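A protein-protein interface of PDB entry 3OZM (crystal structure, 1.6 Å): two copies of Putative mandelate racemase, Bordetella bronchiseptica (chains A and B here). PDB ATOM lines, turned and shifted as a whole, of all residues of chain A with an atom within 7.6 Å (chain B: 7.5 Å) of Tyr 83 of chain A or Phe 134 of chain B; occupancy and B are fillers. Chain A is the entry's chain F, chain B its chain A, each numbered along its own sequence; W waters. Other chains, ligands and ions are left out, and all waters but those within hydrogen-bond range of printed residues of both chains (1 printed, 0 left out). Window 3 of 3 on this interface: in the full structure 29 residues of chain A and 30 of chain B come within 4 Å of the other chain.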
ATOM      1  N   GLN A  72     -34.981  11.797  37.104  1.00  0.00           N
ATOM      2  CA  GLN A  72     -34.668  11.187  35.815  1.00  0.00           C
ATOM      3  C   GLN A  72     -33.715  10.007  35.948  1.00  0.00           C
ATOM      4  O   GLN A  72     -33.587   9.192  35.020  1.00  0.00           O
ATOM      5  CB  GLN A  72     -34.044  12.228  34.885  1.00  0.00           C
ATOM      6  CG  GLN A  72     -34.940  13.415  34.615  1.00  0.00           C
ATOM      7  CD  GLN A  72     -36.191  13.012  33.860  1.00  0.00           C
ATOM      8  OE1 GLN A  72     -36.141  12.178  32.950  1.00  0.00           O
ATOM      9  NE2 GLN A  72     -37.319  13.590  34.235  1.00  0.00           N
ATOM     10  N   GLU A  76     -32.632   3.847  37.188  1.00  0.00           N
ATOM     11  CA  GLU A  76     -31.834   3.629  35.987  1.00  0.00           C
ATOM     12  C   GLU A  76     -30.520   2.922  36.301  1.00  0.00           C
ATOM     13  O   GLU A  76     -29.971   3.058  37.396  1.00  0.00           O
ATOM     14  CB  GLU A  76     -31.523   4.968  35.306  1.00  0.00           C
ATOM     15  CG  GLU A  76     -32.735   5.679  34.695  1.00  0.00           C
ATOM     16  CD  GLU A  76     -33.122   5.111  33.345  1.00  0.00           C
ATOM     17  OE1 GLU A  76     -32.449   4.161  32.874  1.00  0.00           O
ATOM     18  OE2 GLU A  76     -34.099   5.611  32.745  1.00  0.00           O
ATOM     19  N   ASP A  77     -30.014   2.168  35.331  1.00  0.00           N
ATOM     20  CA  ASP A  77     -28.675   1.592  35.425  1.00  0.00           C
ATOM     21  C   ASP A  77     -27.663   2.725  35.257  1.00  0.00           C
ATOM     22  O   ASP A  77     -27.634   3.374  34.204  1.00  0.00           O
ATOM     23  CB  ASP A  77     -28.513   0.549  34.310  1.00  0.00           C
ATOM     24  CG  ASP A  77     -27.142  -0.110  34.291  1.00  0.00           C
ATOM     25  OD1 ASP A  77     -26.258   0.273  35.082  1.00  0.00           O
ATOM     26  OD2 ASP A  77     -26.949  -1.030  33.458  1.00  0.00           O
ATOM     27  N   ALA A  79     -24.587   2.625  34.714  1.00  0.00           N
ATOM     28  CA  ALA A  79     -23.541   2.278  33.755  1.00  0.00           C
ATOM     29  C   ALA A  79     -23.700   3.036  32.430  1.00  0.00           C
ATOM     30  O   ALA A  79     -22.717   3.263  31.722  1.00  0.00           O
ATOM     31  CB  ALA A  79     -23.530   0.766  33.487  1.00  0.00           C
ATOM     32  N   ASN A  80     -24.944   3.375  32.084  1.00  0.00           N
ATOM     33  CA  ASN A  80     -25.257   4.042  30.810  1.00  0.00           C
ATOM     34  C   ASN A  80     -25.142   5.554  30.941  1.00  0.00           C
ATOM     35  O   ASN A  80     -26.132   6.281  30.801  1.00  0.00           O
ATOM     36  CB  ASN A  80     -26.677   3.685  30.331  1.00  0.00           C
ATOM     37  CG  ASN A  80     -26.891   2.177  30.189  1.00  0.00           C
ATOM     38  OD1 ASN A  80     -26.020   1.462  29.705  1.00  0.00           O
ATOM     39  ND2 ASN A  80     -28.061   1.699  30.606  1.00  0.00           N
ATOM     40  N   ILE A  81     -23.934   6.024  31.240  1.00  0.00           N
ATOM     41  CA  ILE A  81     -23.723   7.446  31.471  1.00  0.00           C
ATOM     42  C   ILE A  81     -24.131   8.250  30.241  1.00  0.00           C
ATOM     43  O   ILE A  81     -24.759   9.298  30.358  1.00  0.00           O
ATOM     44  CB  ILE A  81     -22.250   7.730  31.820  1.00  0.00           C
ATOM     45  CG1 ILE A  81     -21.840   6.883  33.031  1.00  0.00           C
ATOM     46  CG2 ILE A  81     -22.039   9.226  32.063  1.00  0.00           C
ATOM     47  CD1 ILE A  81     -20.443   7.205  33.604  1.00  0.00           C
ATOM     48  N   ASN A  82     -23.782   7.757  29.061  1.00  0.00           N
ATOM     49  CA  ASN A  82     -24.113   8.504  27.842  1.00  0.00           C
ATOM     50  C   ASN A  82     -25.616   8.662  27.653  1.00  0.00           C
ATOM     51  O   ASN A  82     -26.119   9.758  27.341  1.00  0.00           O
ATOM     52  CB  ASN A  82     -23.479   7.848  26.611  1.00  0.00           C
ATOM     53  CG  ASN A  82     -21.969   7.969  26.609  1.00  0.00           C
ATOM     54  OD1 ASN A  82     -21.432   9.078  26.640  1.00  0.00           O
ATOM     55  ND2 ASN A  82     -21.276   6.834  26.582  1.00  0.00           N
ATOM     56  N   TYR A  83     -26.332   7.561  27.836  1.00  0.00           N
ATOM     57  CA  TYR A  83     -27.782   7.595  27.777  1.00  0.00           C
ATOM     58  C   TYR A  83     -28.332   8.587  28.789  1.00  0.00           C
ATOM     59  O   TYR A  83     -29.175   9.417  28.457  1.00  0.00           O
ATOM     60  CB  TYR A  83     -28.371   6.217  28.034  1.00  0.00           C
ATOM     61  CG  TYR A  83     -29.857   6.246  28.274  1.00  0.00           C
ATOM     62  CD1 TYR A  83     -30.741   6.455  27.226  1.00  0.00           C
ATOM     63  CD2 TYR A  83     -30.374   6.037  29.544  1.00  0.00           C
ATOM     64  CE1 TYR A  83     -32.101   6.475  27.440  1.00  0.00           C
ATOM     65  CE2 TYR A  83     -31.740   6.056  29.768  1.00  0.00           C
ATOM     66  CZ  TYR A  83     -32.593   6.270  28.713  1.00  0.00           C
ATOM     67  OH  TYR A  83     -33.949   6.289  28.932  1.00  0.00           O
ATOM     68  N   LEU A  84     -27.840   8.518  30.023  1.00  0.00           N
ATOM     69  CA  LEU A  84     -28.389   9.345  31.092  1.00  0.00           C
ATOM     70  C   LEU A  84     -28.102  10.833  30.883  1.00  0.00           C
ATOM     71  O   LEU A  84     -28.919  11.676  31.247  1.00  0.00           O
ATOM     72  CB  LEU A  84     -27.876   8.869  32.456  1.00  0.00           C
ATOM     73  CG  LEU A  84     -28.443   7.534  32.957  1.00  0.00           C
ATOM     74  CD1 LEU A  84     -27.727   7.114  34.237  1.00  0.00           C
ATOM     75  CD2 LEU A  84     -29.954   7.635  33.202  1.00  0.00           C
ATOM     76  N   TRP A  85     -26.947  11.162  30.305  1.00  0.00           N
ATOM     77  CA  TRP A  85     -26.628  12.567  30.053  1.00  0.00           C
ATOM     78  C   TRP A  85     -27.707  13.145  29.137  1.00  0.00           C
ATOM     79  O   TRP A  85     -28.284  14.196  29.408  1.00  0.00           O
ATOM     80  CB  TRP A  85     -25.220  12.726  29.444  1.00  0.00           C
ATOM     81  CG  TRP A  85     -24.717  14.160  29.457  1.00  0.00           C
ATOM     82  CD1 TRP A  85     -23.810  14.708  30.329  1.00  0.00           C
ATOM     83  CD2 TRP A  85     -25.111  15.219  28.572  1.00  0.00           C
ATOM     84  NE1 TRP A  85     -23.620  16.046  30.036  1.00  0.00           N
ATOM     85  CE2 TRP A  85     -24.403  16.379  28.961  1.00  0.00           C
ATOM     86  CE3 TRP A  85     -25.983  15.296  27.482  1.00  0.00           C
ATOM     87  CZ2 TRP A  85     -24.547  17.601  28.300  1.00  0.00           C
ATOM     88  CZ3 TRP A  85     -26.132  16.515  26.830  1.00  0.00           C
ATOM     89  CH2 TRP A  85     -25.419  17.651  27.245  1.00  0.00           C
ATOM     90  N   HIS A  86     -28.022  12.428  28.070  1.00  0.00           N
ATOM     91  CA  HIS A  86     -29.025  12.917  27.129  1.00  0.00           C
ATOM     92  C   HIS A  86     -30.458  12.871  27.657  1.00  0.00           C
ATOM     93  O   HIS A  86     -31.230  13.788  27.406  1.00  0.00           O
ATOM     94  CB  HIS A  86     -28.872  12.221  25.786  1.00  0.00           C
ATOM     95  CG  HIS A  86     -27.615  12.608  25.085  1.00  0.00           C
ATOM     96  ND1 HIS A  86     -27.582  13.571  24.100  1.00  0.00           N
ATOM     97  CD2 HIS A  86     -26.334  12.215  25.274  1.00  0.00           C
ATOM     98  CE1 HIS A  86     -26.337  13.736  23.695  1.00  0.00           C
ATOM     99  NE2 HIS A  86     -25.560  12.923  24.387  1.00  0.00           N
ATOM    100  N   LYS A  87     -30.801  11.828  28.404  1.00  0.00           N
ATOM    101  CA  LYS A  87     -32.114  11.770  29.029  1.00  0.00           C
ATOM    102  C   LYS A  87     -32.329  13.040  29.855  1.00  0.00           C
ATOM    103  O   LYS A  87     -33.355  13.702  29.740  1.00  0.00           O
ATOM    104  CB  LYS A  87     -32.227  10.540  29.937  1.00  0.00           C
ATOM    105  CG  LYS A  87     -33.613  10.365  30.551  1.00  0.00           C
ATOM    106  CD  LYS A  87     -33.664   9.187  31.517  1.00  0.00           C
ATOM    107  CE  LYS A  87     -35.098   8.969  32.000  1.00  0.00           C
ATOM    108  NZ  LYS A  87     -35.139   8.060  33.174  1.00  0.00           N
ATOM    109  N   VAL A  88     -31.337  13.384  30.674  1.00  0.00           N
ATOM    110  CA  VAL A  88     -31.433  14.558  31.543  1.00  0.00           C
ATOM    111  C   VAL A  88     -31.450  15.899  30.788  1.00  0.00           C
ATOM    112  O   VAL A  88     -32.308  16.751  31.045  1.00  0.00           O
ATOM    113  CB  VAL A  88     -30.306  14.549  32.609  1.00  0.00           C
ATOM    114  CG1 VAL A  88     -30.216  15.890  33.332  1.00  0.00           C
ATOM    115  CG2 VAL A  88     -30.529  13.403  33.599  1.00  0.00           C
ATOM    116  N   PHE A  89     -30.520  16.081  29.855  1.00  0.00           N
ATOM    117  CA  PHE A  89     -30.399  17.342  29.129  1.00  0.00           C
ATOM    118  C   PHE A  89     -31.653  17.615  28.296  1.00  0.00           C
ATOM    119  O   PHE A  89     -32.239  18.710  28.340  1.00  0.00           O
ATOM    120  CB  PHE A  89     -29.167  17.304  28.223  1.00  0.00           C
ATOM    121  CG  PHE A  89     -28.959  18.558  27.418  1.00  0.00           C
ATOM    122  CD1 PHE A  89     -28.312  19.649  27.968  1.00  0.00           C
ATOM    123  CD2 PHE A  89     -29.387  18.627  26.101  1.00  0.00           C
ATOM    124  CE1 PHE A  89     -28.104  20.804  27.230  1.00  0.00           C
ATOM    125  CE2 PHE A  89     -29.179  19.776  25.347  1.00  0.00           C
ATOM    126  CZ  PHE A  89     -28.533  20.864  25.912  1.00  0.00           C
ATOM    127  N   HIS A  90     -32.054  16.619  27.515  1.00  0.00           N
ATOM    128  CA  HIS A  90     -33.178  16.794  26.602  1.00  0.00           C
ATOM    129  C   HIS A  90     -34.530  16.700  27.288  1.00  0.00           C
ATOM    130  O   HIS A  90     -35.499  17.308  26.840  1.00  0.00           O
ATOM    131  CB  HIS A  90     -33.086  15.815  25.430  1.00  0.00           C
ATOM    132  CG  HIS A  90     -31.892  16.042  24.564  1.00  0.00           C
ATOM    133  ND1 HIS A  90     -31.740  17.174  23.790  1.00  0.00           N
ATOM    134  CD2 HIS A  90     -30.776  15.298  24.368  1.00  0.00           C
ATOM    135  CE1 HIS A  90     -30.589  17.111  23.145  1.00  0.00           C
ATOM    136  NE2 HIS A  90     -29.984  15.984  23.481  1.00  0.00           N
ATOM    137  N   THR A 285     -18.292  13.739  30.686  1.00  0.00           N
ATOM    138  CA  THR A 285     -18.793  13.336  29.380  1.00  0.00           C
ATOM    139  C   THR A 285     -18.658  14.475  28.361  1.00  0.00           C
ATOM    140  O   THR A 285     -18.171  14.275  27.238  1.00  0.00           O
ATOM    141  CB  THR A 285     -20.258  12.897  29.492  1.00  0.00           C
ATOM    142  OG1 THR A 285     -20.353  11.813  30.433  1.00  0.00           O
ATOM    143  CG2 THR A 285     -20.808  12.441  28.138  1.00  0.00           C
ATOM    144  N   TYR B 127     -17.514  -0.833  25.357  1.00  0.00           N
ATOM    145  CA  TYR B 127     -18.542   0.208  25.432  1.00  0.00           C
ATOM    146  C   TYR B 127     -18.755   0.709  26.864  1.00  0.00           C
ATOM    147  O   TYR B 127     -19.146   1.855  27.070  1.00  0.00           O
ATOM    148  CB  TYR B 127     -19.867  -0.220  24.782  1.00  0.00           C
ATOM    149  CG  TYR B 127     -20.684  -1.249  25.541  1.00  0.00           C
ATOM    150  CD1 TYR B 127     -21.548  -0.870  26.564  1.00  0.00           C
ATOM    151  CD2 TYR B 127     -20.613  -2.602  25.210  1.00  0.00           C
ATOM    152  CE1 TYR B 127     -22.295  -1.809  27.255  1.00  0.00           C
ATOM    153  CE2 TYR B 127     -21.368  -3.550  25.902  1.00  0.00           C
ATOM    154  CZ  TYR B 127     -22.206  -3.143  26.912  1.00  0.00           C
ATOM    155  OH  TYR B 127     -22.956  -4.080  27.591  1.00  0.00           O
ATOM    156  N   GLY B 131     -18.190   5.173  28.688  1.00  0.00           N
ATOM    157  CA  GLY B 131     -19.335   5.832  29.279  1.00  0.00           C
ATOM    158  C   GLY B 131     -20.632   5.058  29.176  1.00  0.00           C
ATOM    159  O   GLY B 131     -21.690   5.569  29.551  1.00  0.00           O
ATOM    160  N   GLY B 132     -20.562   3.825  28.686  1.00  0.00           N
ATOM    161  CA  GLY B 132     -21.749   2.993  28.599  1.00  0.00           C
ATOM    162  C   GLY B 132     -22.606   3.288  27.382  1.00  0.00           C
ATOM    163  O   GLY B 132     -22.288   4.143  26.566  1.00  0.00           O
ATOM    164  N   LYS B 133     -23.714   2.575  27.262  1.00  0.00           N
ATOM    165  CA  LYS B 133     -24.574   2.729  26.105  1.00  0.00           C
ATOM    166  C   LYS B 133     -25.289   4.071  26.052  1.00  0.00           C
ATOM    167  O   LYS B 133     -25.663   4.645  27.082  1.00  0.00           O
ATOM    168  CB  LYS B 133     -25.595   1.603  26.055  1.00  0.00           C
ATOM    169  CG  LYS B 133     -24.981   0.275  25.700  1.00  0.00           C
ATOM    170  CD  LYS B 133     -26.017  -0.834  25.565  1.00  0.00           C
ATOM    171  CE  LYS B 133     -25.320  -2.131  25.156  1.00  0.00           C
ATOM    172  NZ  LYS B 133     -26.206  -3.317  25.257  1.00  0.00           N
ATOM    173  N   PHE B 134     -25.449   4.569  24.832  1.00  0.00           N
ATOM    174  CA  PHE B 134     -26.481   5.540  24.536  1.00  0.00           C
ATOM    175  C   PHE B 134     -27.689   4.794  23.962  1.00  0.00           C
ATOM    176  O   PHE B 134     -28.825   5.009  24.391  1.00  0.00           O
ATOM    177  CB  PHE B 134     -25.991   6.580  23.520  1.00  0.00           C
ATOM    178  CG  PHE B 134     -27.076   7.502  23.056  1.00  0.00           C
ATOM    179  CD1 PHE B 134     -27.327   8.693  23.725  1.00  0.00           C
ATOM    180  CD2 PHE B 134     -27.888   7.151  21.986  1.00  0.00           C
ATOM    181  CE1 PHE B 134     -28.345   9.530  23.310  1.00  0.00           C
ATOM    182  CE2 PHE B 134     -28.913   7.984  21.568  1.00  0.00           C
ATOM    183  CZ  PHE B 134     -29.143   9.170  22.233  1.00  0.00           C
ATOM    184  N   HIS B 135     -27.425   3.922  22.985  1.00  0.00           N
ATOM    185  CA  HIS B 135     -28.470   3.140  22.316  1.00  0.00           C
ATOM    186  C   HIS B 135     -28.781   1.882  23.120  1.00  0.00           C
ATOM    187  O   HIS B 135     -28.392   0.772  22.752  1.00  0.00           O
ATOM    188  CB  HIS B 135     -28.046   2.789  20.885  1.00  0.00           C
ATOM    189  CG  HIS B 135     -27.864   3.991  20.011  1.00  0.00           C
ATOM    190  ND1 HIS B 135     -28.928   4.683  19.469  1.00  0.00           N
ATOM    191  CD2 HIS B 135     -26.747   4.652  19.622  1.00  0.00           C
ATOM    192  CE1 HIS B 135     -28.471   5.705  18.765  1.00  0.00           C
ATOM    193  NE2 HIS B 135     -27.153   5.715  18.847  1.00  0.00           N
ATOM    194  N   THR B 136     -29.478   2.066  24.233  1.00  0.00           N
ATOM    195  CA  THR B 136     -29.718   0.963  25.150  1.00  0.00           C
ATOM    196  C   THR B 136     -30.551  -0.150  24.518  1.00  0.00           C
ATOM    197  O   THR B 136     -30.387  -1.315  24.873  1.00  0.00           O
ATOM    198  CB  THR B 136     -30.398   1.447  26.441  1.00  0.00           C
ATOM    199  OG1 THR B 136     -31.649   2.048  26.112  1.00  0.00           O
ATOM    200  CG2 THR B 136     -29.518   2.477  27.153  1.00  0.00           C
ATOM    201  N   ARG B 137     -31.435   0.209  23.587  1.00  0.00           N
ATOM    202  CA  ARG B 137     -32.330  -0.767  22.959  1.00  0.00           C
ATOM    203  C   ARG B 137     -31.671  -1.508  21.804  1.00  0.00           C
ATOM    204  O   ARG B 137     -32.167  -2.539  21.345  1.00  0.00           O
ATOM    205  CB  ARG B 137     -33.600  -0.088  22.437  1.00  0.00           C
ATOM    206  CG  ARG B 137     -34.403   0.664  23.485  1.00  0.00           C
ATOM    207  CD  ARG B 137     -35.015  -0.279  24.505  1.00  0.00           C
ATOM    208  NE  ARG B 137     -35.936   0.421  25.399  1.00  0.00           N
ATOM    209  CZ  ARG B 137     -35.574   1.014  26.533  1.00  0.00           C
ATOM    210  NH1 ARG B 137     -34.305   0.993  26.922  1.00  0.00           N
ATOM    211  NH2 ARG B 137     -36.483   1.630  27.280  1.00  0.00           N
ATOM    212  N   GLY B 138     -30.563  -0.971  21.310  1.00  0.00           N
ATOM    213  CA  GLY B 138     -29.879  -1.585  20.186  1.00  0.00           C
ATOM    214  C   GLY B 138     -29.541  -0.558  19.131  1.00  0.00           C
ATOM    215  O   GLY B 138     -30.009   0.580  19.187  1.00  0.00           O
ATOM    216  N   VAL B 139     -28.741  -0.985  18.161  1.00  0.00           N
ATOM    217  CA  VAL B 139     -28.230  -0.114  17.107  1.00  0.00           C
ATOM    218  C   VAL B 139     -28.822  -0.470  15.738  1.00  0.00           C
ATOM    219  O   VAL B 139     -28.690  -1.600  15.269  1.00  0.00           O
ATOM    220  CB  VAL B 139     -26.692  -0.212  17.058  1.00  0.00           C
ATOM    221  CG1 VAL B 139     -26.123   0.531  15.863  1.00  0.00           C
ATOM    222  CG2 VAL B 139     -26.102   0.312  18.366  1.00  0.00           C
ATOM    223  N   HIS B 317     -18.964  -1.019  19.384  1.00  0.00           N
ATOM    224  CA  HIS B 317     -18.842  -0.558  20.766  1.00  0.00           C
ATOM    225  C   HIS B 317     -18.971   0.961  20.827  1.00  0.00           C
ATOM    226  O   HIS B 317     -19.682   1.502  21.672  1.00  0.00           O
ATOM    227  CB  HIS B 317     -17.517  -1.004  21.398  1.00  0.00           C
ATOM    228  CG  HIS B 317     -17.505  -2.431  21.846  1.00  0.00           C
ATOM    229  ND1 HIS B 317     -18.002  -2.835  23.068  1.00  0.00           N
ATOM    230  CD2 HIS B 317     -17.043  -3.548  21.239  1.00  0.00           C
ATOM    231  CE1 HIS B 317     -17.855  -4.143  23.188  1.00  0.00           C
ATOM    232  NE2 HIS B 317     -17.275  -4.599  22.091  1.00  0.00           N
ATOM    233  N   LEU B 318     -18.308   1.652  19.904  1.00  0.00           N
ATOM    234  CA  LEU B 318     -18.323   3.115  19.890  1.00  0.00           C
ATOM    235  C   LEU B 318     -19.685   3.640  19.489  1.00  0.00           C
ATOM    236  O   LEU B 318     -20.215   4.584  20.091  1.00  0.00           O
ATOM    237  CB  LEU B 318     -17.272   3.658  18.915  1.00  0.00           C
ATOM    238  CG  LEU B 318     -15.828   3.753  19.412  1.00  0.00           C
ATOM    239  CD1 LEU B 318     -15.341   2.428  20.018  1.00  0.00           C
ATOM    240  CD2 LEU B 318     -14.920   4.174  18.276  1.00  0.00           C
ATOM    241  N   VAL B 319     -20.246   3.045  18.444  1.00  0.00           N
ATOM    242  CA  VAL B 319     -21.551   3.474  17.968  1.00  0.00           C
ATOM    243  C   VAL B 319     -22.619   3.301  19.056  1.00  0.00           C
ATOM    244  O   VAL B 319     -23.463   4.174  19.256  1.00  0.00           O
ATOM    245  CB  VAL B 319     -21.956   2.722  16.689  1.00  0.00           C
ATOM    246  CG1 VAL B 319     -23.445   2.911  16.420  1.00  0.00           C
ATOM    247  CG2 VAL B 319     -21.112   3.200  15.508  1.00  0.00           C
ATOM    248  N   ALA B 320     -22.569   2.181  19.769  1.00  0.00           N
ATOM    249  CA  ALA B 320     -23.543   1.932  20.836  1.00  0.00           C
ATOM    250  C   ALA B 320     -23.469   2.983  21.937  1.00  0.00           C
ATOM    251  O   ALA B 320     -24.475   3.309  22.573  1.00  0.00           O
ATOM    252  CB  ALA B 320     -23.335   0.526  21.421  1.00  0.00           C
ATOM    253  N   ALA B 321     -22.268   3.509  22.157  1.00  0.00           N
ATOM    254  CA  ALA B 321     -22.024   4.460  23.226  1.00  0.00           C
ATOM    255  C   ALA B 321     -22.278   5.894  22.776  1.00  0.00           C
ATOM    256  O   ALA B 321     -22.318   6.802  23.598  1.00  0.00           O
ATOM    257  CB  ALA B 321     -20.581   4.323  23.727  1.00  0.00           C
ATOM    258  N   SER B 322     -22.425   6.089  21.471  1.00  0.00           N
ATOM    259  CA  SER B 322     -22.562   7.426  20.881  1.00  0.00           C
ATOM    260  C   SER B 322     -24.011   7.880  20.646  1.00  0.00           C
ATOM    261  O   SER B 322     -24.859   7.101  20.202  1.00  0.00           O
ATOM    262  CB  SER B 322     -21.789   7.476  19.557  1.00  0.00           C
ATOM    263  OG  SER B 322     -22.093   8.674  18.874  1.00  0.00           O
ATOM    264  N   PRO B 323     -24.302   9.160  20.936  1.00  0.00           N
ATOM    265  CA  PRO B 323     -25.637   9.736  20.713  1.00  0.00           C
ATOM    266  C   PRO B 323     -25.986   9.988  19.240  1.00  0.00           C
ATOM    267  O   PRO B 323     -27.122  10.371  18.949  1.00  0.00           O
ATOM    268  CB  PRO B 323     -25.589  11.056  21.497  1.00  0.00           C
ATOM    269  CG  PRO B 323     -24.145  11.399  21.564  1.00  0.00           C
ATOM    270  CD  PRO B 323     -23.427  10.078  21.688  1.00  0.00           C
ATOM    271  N   HIS B 324     -25.052   9.778  18.317  1.00  0.00           N
ATOM    272  CA  HIS B 324     -25.402   9.920  16.896  1.00  0.00           C
ATOM    273  C   HIS B 324     -26.471   8.893  16.531  1.00  0.00           C
ATOM    274  O   HIS B 324     -26.325   7.709  16.848  1.00  0.00           O
ATOM    275  CB  HIS B 324     -24.180   9.688  16.007  1.00  0.00           C
ATOM    276  CG  HIS B 324     -23.137  10.756  16.115  1.00  0.00           C
ATOM    277  ND1 HIS B 324     -23.343  12.044  15.670  1.00  0.00           N
ATOM    278  CD2 HIS B 324     -21.881  10.726  16.620  1.00  0.00           C
ATOM    279  CE1 HIS B 324     -22.257  12.760  15.897  1.00  0.00           C
ATOM    280  NE2 HIS B 324     -21.357  11.986  16.476  1.00  0.00           N
ATOM    281  N   PRO B 325     -27.548   9.332  15.870  1.00  0.00           N
ATOM    282  CA  PRO B 325     -28.513   8.373  15.313  1.00  0.00           C
ATOM    283  C   PRO B 325     -27.789   7.324  14.490  1.00  0.00           C
ATOM    284  O   PRO B 325     -26.942   7.663  13.663  1.00  0.00           O
ATOM    285  CB  PRO B 325     -29.373   9.243  14.408  1.00  0.00           C
ATOM    286  CG  PRO B 325     -29.384  10.571  15.118  1.00  0.00           C
ATOM    287  CD  PRO B 325     -28.010  10.725  15.728  1.00  0.00           C
ATOM    288  N   ALA B 326     -28.120   6.063  14.718  1.00  0.00           N
ATOM    289  CA  ALA B 326     -27.341   4.973  14.144  1.00  0.00           C
ATOM    290  C   ALA B 326     -27.759   4.627  12.723  1.00  0.00           C
ATOM    291  O   ALA B 326     -28.936   4.681  12.374  1.00  0.00           O
ATOM    292  CB  ALA B 326     -27.442   3.746  15.029  1.00  0.00           C
HETATM  293  O   HOH W   1     -23.705   0.695  29.411  1.00  0.00           O
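Water W1 bridges the side-chain amide oxygen (OD1) of Asn 80 of chain A and the backbone NH (N) of Lys 133 of chain B.
Printed residues of chain B that touch a printed residue of chain A: Gly 131, Gly 132, Lys 133, Phe 134, Thr 136, Ala 321 and Pro 323.
Among the printed residues, 16 pairs touch across the chains.
Among the printed residues, no Asp or Glu carboxylate lies within 4 Å of a Lys or Arg side-chain nitrogen of the other chain.
No position is printed for both chains.
The backbone carbonyl oxygen (O) of Ala 321 of chain B sits at hydrogen-bond distance from the side-chain amide nitrogen (ND2) of Asn 82 of chain A (3.2 Å).
The backbone carbonyl oxygen (O) of Lys 133 of chain B lies within hydrogen-bond range of the backbone NH (N) of Tyr 83 of chain A, 3.1 Å away.
The backbone carbonyl oxygen of Gly 131 of chain B lies close to the backbone carbonyl oxygen of Ala 79 of chain A.
The backbone carbonyl oxygen (O) of Gly 132 of chain B sits at hydrogen-bond distance from the side-chain amide nitrogen (ND2) of Asn 82 of chain A (2.9 Å).
The backbone carbonyl oxygen of Gly 131 of chain B lies within hydrogen-bond range of the backbone NH of Ile 81 of chain A, 2.8 Å away.
The backbone carbonyl oxygen (O) of Gly 131 of chain B lies within hydrogen-bond range of the backbone NH (N) of Asn 82 of chain A, at 3.1 Å.
OD1 of Asp 77 of chain A sits at hydrogen-bond distance from N of Ala 79 of chain A (2.9 Å).
ND1 of His 86 of chain A is in hydrogen-bond range of NE2 of His 90 of chain A (3.5 Å).
The side-chain hydroxyl (OG1) of Thr 136 of chain B sits at hydrogen-bond distance from the guanidinium group (NH1) of Arg 137 of chain B, 3.0 Å away.
O of Tyr 127 of chain B lies within hydrogen-bond range of N of Gly 132 of chain B (2.9 Å).
The backbone NH (N) of Phe 134 of chain B is in hydrogen-bond range of the backbone carbonyl oxygen (O) of Ala 320 of chain B, 2.8 Å away.
Ala 79 of chain A touches Gly 132 of chain B.
Asn 80 of chain A touches Gly 131 of chain B (C to O, 3.7 Å).
Asn 80 of chain A touches Lys 133 of chain B.
Asn 80 of chain A touches Thr 136 of chain B (ND2 to CG2, 3.8 Å).
CB of Asn 82 of chain A touches O of Lys 133 of chain B, at 3.9 Å.
Phe 134 of chain B touches Asn 82 of chain A.
Tyr 83 of chain A touches Phe 134 of chain B.
CG of Tyr 83 of chain A touches CG2 of Thr 136 of chain B, at 3.9 Å.
His 86 of chain A touches Phe 134 of chain B (CG to CE1, 3.6 Å).
NE2 of His 86 of chain A touches CB of Pro 323 of chain B, 3.4 Å away.
Of chain A, only Asn 82, Tyr 83 and His 86 come within 4 Å of Phe 134 of chain B.
Printed residues of chain A within 4 Å of Thr 136 of chain B: Asn 80 and Tyr 83.
Of the printed residues of chain A, Lys 133 of chain B touches Asn 80, Asn 82 and Tyr 83.
Printed residues of chain B within 4 Å of Ile 81 of chain A: Gly 131.
Of the printed residues of chain A, Ala 321 of chain B touches Asn 82.
Of the printed residues of chain B, Asn 80 of chain A touches Gly 131 (3.7 Å), Lys 133 (3.5 Å) and Thr 136 (3.8 Å).
Gln 72 of chain A touches none of the printed residues of chain B.
The nearest residue of chain A that does not touch Phe 134 of chain B is Asn 80 of chain A (5.7 Å).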
